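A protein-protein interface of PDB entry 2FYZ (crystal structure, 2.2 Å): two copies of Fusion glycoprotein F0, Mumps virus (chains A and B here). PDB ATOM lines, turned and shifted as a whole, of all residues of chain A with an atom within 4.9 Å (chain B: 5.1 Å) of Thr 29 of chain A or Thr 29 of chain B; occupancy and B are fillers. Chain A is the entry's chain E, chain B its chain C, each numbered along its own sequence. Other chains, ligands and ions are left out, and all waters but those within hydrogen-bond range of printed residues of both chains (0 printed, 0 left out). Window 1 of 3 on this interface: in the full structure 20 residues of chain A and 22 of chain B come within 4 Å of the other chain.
The side-chain amide oxygen (OD1) of Asn 30 of chain B sits at hydrogen-bond distance from the side-chain hydroxyl (OG1) of Thr 29 of chain A, 2.7 Å away.
The side-chain hydroxyl of Thr 29 of chain B lies within hydrogen-bond range of the backbone carbonyl oxygen of Ser 25 of chain B (3.1 Å). The side-chain hydroxyl (OG1) of Thr 29 of chain A sits at hydrogen-bond distance from the backbone carbonyl oxygen (O) of Ser 25 of chain A (3.2 Å). The backbone carbonyl oxygen (O) of Ile 26 of chain A lies close to the side-chain amide nitrogen (ND2) of Asn 30 of chain A (3.5 Å).
Among the printed residues, merely in contact across the chains: Ser 25 of chain A with Ile 26 of chain B, Val 33 of chain A with Val 33 of chain B, Ile 26 of chain A with Ile 26 of chain B and Thr 29 of chain A with Thr 29 of chain B.
Printed residues of chain B within 4 Å of Thr 29 of chain A: Thr 29 and Asn 30. Printed residues of chain A within 4 Å of Thr 29 of chain B: Thr 29. Of the printed residues of chain B, Ser 25 of chain A touches Ile 26. Of the printed residues of chain A, Asn 30 of chain B touches Thr 29. Arg 31 of chain B touches none of the printed residues of chain A. The nearest printed residue of chain A that does not touch Asn 30 of chain B is Ser 25 of chain A (4.8 Å).
Of the 9 printed residues of chain A, 4 touch a printed residue of chain B. Hydrophobic or aromatic side chains of chain A within 4 Å of the printed part of chain B: Ile 26 and Val 33. Of the 10 printed residues of chain B, 4 touch a printed residue of chain A. Along chain B the printed residues that touch a printed residue of chain A span positions 26 to 33. Among the printed residues, 5 pairs touch across the chains. Among the printed residues, no Asp or Glu carboxylate lies within 4 Å of a Lys or Arg side-chain nitrogen of the other chain.
Ser 25 of chain A touches Ile 26 of chain B, but with the chains exchanged Ile 26 of chain A does not touch Ser 25 of chain B (8.2 Å). Ile 26 of chain B touches its own counterpart, Ile 26 of chain A. Thr 29 of chain A touches its own counterpart, Thr 29 of chain B. Val 33 of chain B touches its own counterpart, Val 33 of chain A. 9 positions are printed for both chains.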
ATOM      1  N   SER A  25     -13.613 -18.231   3.625  1.00  0.00           N
ATOM      2  CA  SER A  25     -13.161 -18.530   4.977  1.00  0.00           C
ATOM      3  C   SER A  25     -14.257 -18.240   5.993  1.00  0.00           C
ATOM      4  O   SER A  25     -14.596 -19.097   6.807  1.00  0.00           O
ATOM      5  CB  SER A  25     -11.920 -17.707   5.337  1.00  0.00           C
ATOM      6  OG  SER A  25     -11.562 -17.915   6.699  1.00  0.00           O
ATOM      7  N   ILE A  26     -14.807 -17.032   5.940  1.00  0.00           N
ATOM      8  CA  ILE A  26     -15.862 -16.640   6.864  1.00  0.00           C
ATOM      9  C   ILE A  26     -17.055 -17.587   6.778  1.00  0.00           C
ATOM     10  O   ILE A  26     -17.603 -17.990   7.801  1.00  0.00           O
ATOM     11  CB  ILE A  26     -16.328 -15.203   6.591  1.00  0.00           C
ATOM     12  CG1 ILE A  26     -15.154 -14.243   6.792  1.00  0.00           C
ATOM     13  CG2 ILE A  26     -17.462 -14.827   7.546  1.00  0.00           C
ATOM     14  CD1 ILE A  26     -15.419 -12.845   6.251  1.00  0.00           C
ATOM     15  N   GLN A  27     -17.446 -17.956   5.564  1.00  0.00           N
ATOM     16  CA  GLN A  27     -18.567 -18.870   5.389  1.00  0.00           C
ATOM     17  C   GLN A  27     -18.266 -20.233   6.028  1.00  0.00           C
ATOM     18  O   GLN A  27     -19.144 -20.860   6.620  1.00  0.00           O
ATOM     19  CB  GLN A  27     -18.887 -19.042   3.898  1.00  0.00           C
ATOM     20  CG  GLN A  27     -19.593 -17.838   3.275  1.00  0.00           C
ATOM     21  CD  GLN A  27     -19.759 -17.967   1.764  1.00  0.00           C
ATOM     22  OE1 GLN A  27     -20.543 -17.245   1.149  1.00  0.00           O
ATOM     23  NE2 GLN A  27     -19.012 -18.881   1.163  1.00  0.00           N
ATOM     24  N   ALA A  28     -17.024 -20.691   5.914  1.00  0.00           N
ATOM     25  CA  ALA A  28     -16.671 -21.972   6.498  1.00  0.00           C
ATOM     26  C   ALA A  28     -16.663 -21.825   8.020  1.00  0.00           C
ATOM     27  O   ALA A  28     -17.017 -22.752   8.751  1.00  0.00           O
ATOM     28  CB  ALA A  28     -15.310 -22.433   5.985  1.00  0.00           C
ATOM     29  N   THR A  29     -16.287 -20.649   8.499  1.00  0.00           N
ATOM     30  CA  THR A  29     -16.264 -20.421   9.935  1.00  0.00           C
ATOM     31  C   THR A  29     -17.688 -20.380  10.487  1.00  0.00           C
ATOM     32  O   THR A  29     -17.943 -20.874  11.584  1.00  0.00           O
ATOM     33  CB  THR A  29     -15.549 -19.115  10.270  1.00  0.00           C
ATOM     34  OG1 THR A  29     -14.158 -19.258   9.962  1.00  0.00           O
ATOM     35  CG2 THR A  29     -15.713 -18.771  11.743  1.00  0.00           C
ATOM     36  N   ASN A  30     -18.614 -19.795   9.728  1.00  0.00           N
ATOM     37  CA  ASN A  30     -19.996 -19.735  10.181  1.00  0.00           C
ATOM     38  C   ASN A  30     -20.558 -21.143  10.269  1.00  0.00           C
ATOM     39  O   ASN A  30     -21.332 -21.449  11.173  1.00  0.00           O
ATOM     40  CB  ASN A  30     -20.862 -18.892   9.237  1.00  0.00           C
ATOM     41  CG  ASN A  30     -20.553 -17.415   9.331  1.00  0.00           C
ATOM     42  OD1 ASN A  30     -20.128 -16.933  10.380  1.00  0.00           O
ATOM     43  ND2 ASN A  30     -20.781 -16.684   8.240  1.00  0.00           N
ATOM     44  N   ARG A  31     -20.172 -21.998   9.324  1.00  0.00           N
ATOM     45  CA  ARG A  31     -20.640 -23.378   9.334  1.00  0.00           C
ATOM     46  C   ARG A  31     -20.116 -24.094  10.582  1.00  0.00           C
ATOM     47  O   ARG A  31     -20.834 -24.864  11.212  1.00  0.00           O
ATOM     48  CB  ARG A  31     -20.183 -24.104   8.063  1.00  0.00           C
ATOM     49  CG  ARG A  31     -21.080 -23.846   6.852  1.00  0.00           C
ATOM     50  CD  ARG A  31     -20.438 -24.320   5.557  1.00  0.00           C
ATOM     51  NE  ARG A  31     -19.539 -23.301   5.016  1.00  0.00           N
ATOM     52  CZ  ARG A  31     -18.676 -23.496   4.023  1.00  0.00           C
ATOM     53  NH1 ARG A  31     -18.575 -24.682   3.439  1.00  0.00           N
ATOM     54  NH2 ARG A  31     -17.904 -22.498   3.621  1.00  0.00           N
ATOM     55  N   ALA A  32     -18.866 -23.833  10.941  1.00  0.00           N
ATOM     56  CA  ALA A  32     -18.286 -24.450  12.133  1.00  0.00           C
ATOM     57  C   ALA A  32     -19.045 -23.972  13.374  1.00  0.00           C
ATOM     58  O   ALA A  32     -19.346 -24.762  14.263  1.00  0.00           O
ATOM     59  CB  ALA A  32     -16.804 -24.095  12.243  1.00  0.00           C
ATOM     60  N   VAL A  33     -19.353 -22.677  13.426  1.00  0.00           N
ATOM     61  CA  VAL A  33     -20.093 -22.121  14.550  1.00  0.00           C
ATOM     62  C   VAL A  33     -21.468 -22.790  14.613  1.00  0.00           C
ATOM     63  O   VAL A  33     -21.950 -23.151  15.696  1.00  0.00           O
ATOM     64  CB  VAL A  33     -20.286 -20.584  14.408  1.00  0.00           C
ATOM     65  CG1 VAL A  33     -21.141 -20.050  15.562  1.00  0.00           C
ATOM     66  CG2 VAL A  33     -18.928 -19.888  14.391  1.00  0.00           C
ATOM     67  N   ASN B  24      -6.109 -11.998  10.612  1.00  0.00           N
ATOM     68  CA  ASN B  24      -5.782 -12.261  12.003  1.00  0.00           C
ATOM     69  C   ASN B  24      -7.078 -12.400  12.799  1.00  0.00           C
ATOM     70  O   ASN B  24      -7.206 -13.282  13.652  1.00  0.00           O
ATOM     71  CB  ASN B  24      -4.936 -11.128  12.591  1.00  0.00           C
ATOM     72  CG  ASN B  24      -3.554 -11.045  11.967  1.00  0.00           C
ATOM     73  OD1 ASN B  24      -2.965 -12.059  11.593  1.00  0.00           O
ATOM     74  ND2 ASN B  24      -3.021  -9.835  11.871  1.00  0.00           N
ATOM     75  N   SER B  25      -8.038 -11.527  12.507  1.00  0.00           N
ATOM     76  CA  SER B  25      -9.331 -11.547  13.184  1.00  0.00           C
ATOM     77  C   SER B  25      -9.988 -12.922  13.033  1.00  0.00           C
ATOM     78  O   SER B  25     -10.356 -13.565  14.026  1.00  0.00           O
ATOM     79  CB  SER B  25     -10.237 -10.450  12.607  1.00  0.00           C
ATOM     80  OG  SER B  25     -11.523 -10.480  13.194  1.00  0.00           O
ATOM     81  N   ILE B  26     -10.111 -13.381  11.792  1.00  0.00           N
ATOM     82  CA  ILE B  26     -10.707 -14.686  11.520  1.00  0.00           C
ATOM     83  C   ILE B  26      -9.895 -15.816  12.164  1.00  0.00           C
ATOM     84  O   ILE B  26     -10.450 -16.802  12.641  1.00  0.00           O
ATOM     85  CB  ILE B  26     -10.823 -14.938   9.997  1.00  0.00           C
ATOM     86  CG1 ILE B  26     -11.699 -13.856   9.360  1.00  0.00           C
ATOM     87  CG2 ILE B  26     -11.463 -16.294   9.742  1.00  0.00           C
ATOM     88  CD1 ILE B  26     -11.782 -13.934   7.839  1.00  0.00           C
ATOM     89  N   GLN B  27      -8.578 -15.676  12.182  1.00  0.00           N
ATOM     90  CA  GLN B  27      -7.748 -16.700  12.803  1.00  0.00           C
ATOM     91  C   GLN B  27      -8.045 -16.747  14.303  1.00  0.00           C
ATOM     92  O   GLN B  27      -7.975 -17.805  14.929  1.00  0.00           O
ATOM     93  CB  GLN B  27      -6.266 -16.406  12.553  1.00  0.00           C
ATOM     94  CG  GLN B  27      -5.824 -16.730  11.133  1.00  0.00           C
ATOM     95  CD  GLN B  27      -4.426 -16.227  10.808  1.00  0.00           C
ATOM     96  OE1 GLN B  27      -3.685 -16.866  10.062  1.00  0.00           O
ATOM     97  NE2 GLN B  27      -4.067 -15.069  11.349  1.00  0.00           N
ATOM     98  N   ALA B  28      -8.396 -15.597  14.871  1.00  0.00           N
ATOM     99  CA  ALA B  28      -8.715 -15.522  16.289  1.00  0.00           C
ATOM    100  C   ALA B  28     -10.122 -16.102  16.503  1.00  0.00           C
ATOM    101  O   ALA B  28     -10.365 -16.854  17.451  1.00  0.00           O
ATOM    102  CB  ALA B  28      -8.646 -14.063  16.765  1.00  0.00           C
ATOM    103  N   THR B  29     -11.037 -15.758  15.604  1.00  0.00           N
ATOM    104  CA  THR B  29     -12.400 -16.249  15.673  1.00  0.00           C
ATOM    105  C   THR B  29     -12.415 -17.768  15.571  1.00  0.00           C
ATOM    106  O   THR B  29     -13.162 -18.439  16.275  1.00  0.00           O
ATOM    107  CB  THR B  29     -13.242 -15.667  14.541  1.00  0.00           C
ATOM    108  OG1 THR B  29     -13.331 -14.245  14.709  1.00  0.00           O
ATOM    109  CG2 THR B  29     -14.642 -16.272  14.546  1.00  0.00           C
ATOM    110  N   ASN B  30     -11.580 -18.317  14.701  1.00  0.00           N
ATOM    111  CA  ASN B  30     -11.530 -19.764  14.555  1.00  0.00           C
ATOM    112  C   ASN B  30     -11.078 -20.426  15.845  1.00  0.00           C
ATOM    113  O   ASN B  30     -11.623 -21.454  16.242  1.00  0.00           O
ATOM    114  CB  ASN B  30     -10.610 -20.161  13.398  1.00  0.00           C
ATOM    115  CG  ASN B  30     -11.249 -19.904  12.052  1.00  0.00           C
ATOM    116  OD1 ASN B  30     -12.461 -19.735  11.974  1.00  0.00           O
ATOM    117  ND2 ASN B  30     -10.446 -19.892  10.980  1.00  0.00           N
ATOM    118  N   ARG B  31     -10.099 -19.822  16.510  1.00  0.00           N
ATOM    119  CA  ARG B  31      -9.598 -20.365  17.771  1.00  0.00           C
ATOM    120  C   ARG B  31     -10.702 -20.358  18.819  1.00  0.00           C
ATOM    121  O   ARG B  31     -10.799 -21.275  19.635  1.00  0.00           O
ATOM    122  CB  ARG B  31      -8.402 -19.548  18.269  1.00  0.00           C
ATOM    123  N   ALA B  32     -11.535 -19.322  18.803  1.00  0.00           N
ATOM    124  CA  ALA B  32     -12.626 -19.234  19.765  1.00  0.00           C
ATOM    125  C   ALA B  32     -13.638 -20.360  19.526  1.00  0.00           C
ATOM    126  O   ALA B  32     -14.055 -21.038  20.463  1.00  0.00           O
ATOM    127  CB  ALA B  32     -13.309 -17.855  19.675  1.00  0.00           C
ATOM    128  N   VAL B  33     -14.023 -20.565  18.272  1.00  0.00           N
ATOM    129  CA  VAL B  33     -14.978 -21.616  17.934  1.00  0.00           C
ATOM    130  C   VAL B  33     -14.459 -22.978  18.396  1.00  0.00           C
ATOM    131  O   VAL B  33     -15.215 -23.794  18.940  1.00  0.00           O
ATOM    132  CB  VAL B  33     -15.247 -21.641  16.416  1.00  0.00           C
ATOM    133  CG1 VAL B  33     -16.175 -22.799  16.053  1.00  0.00           C
ATOM    134  CG2 VAL B  33     -15.869 -20.314  16.000  1.00  0.00           C
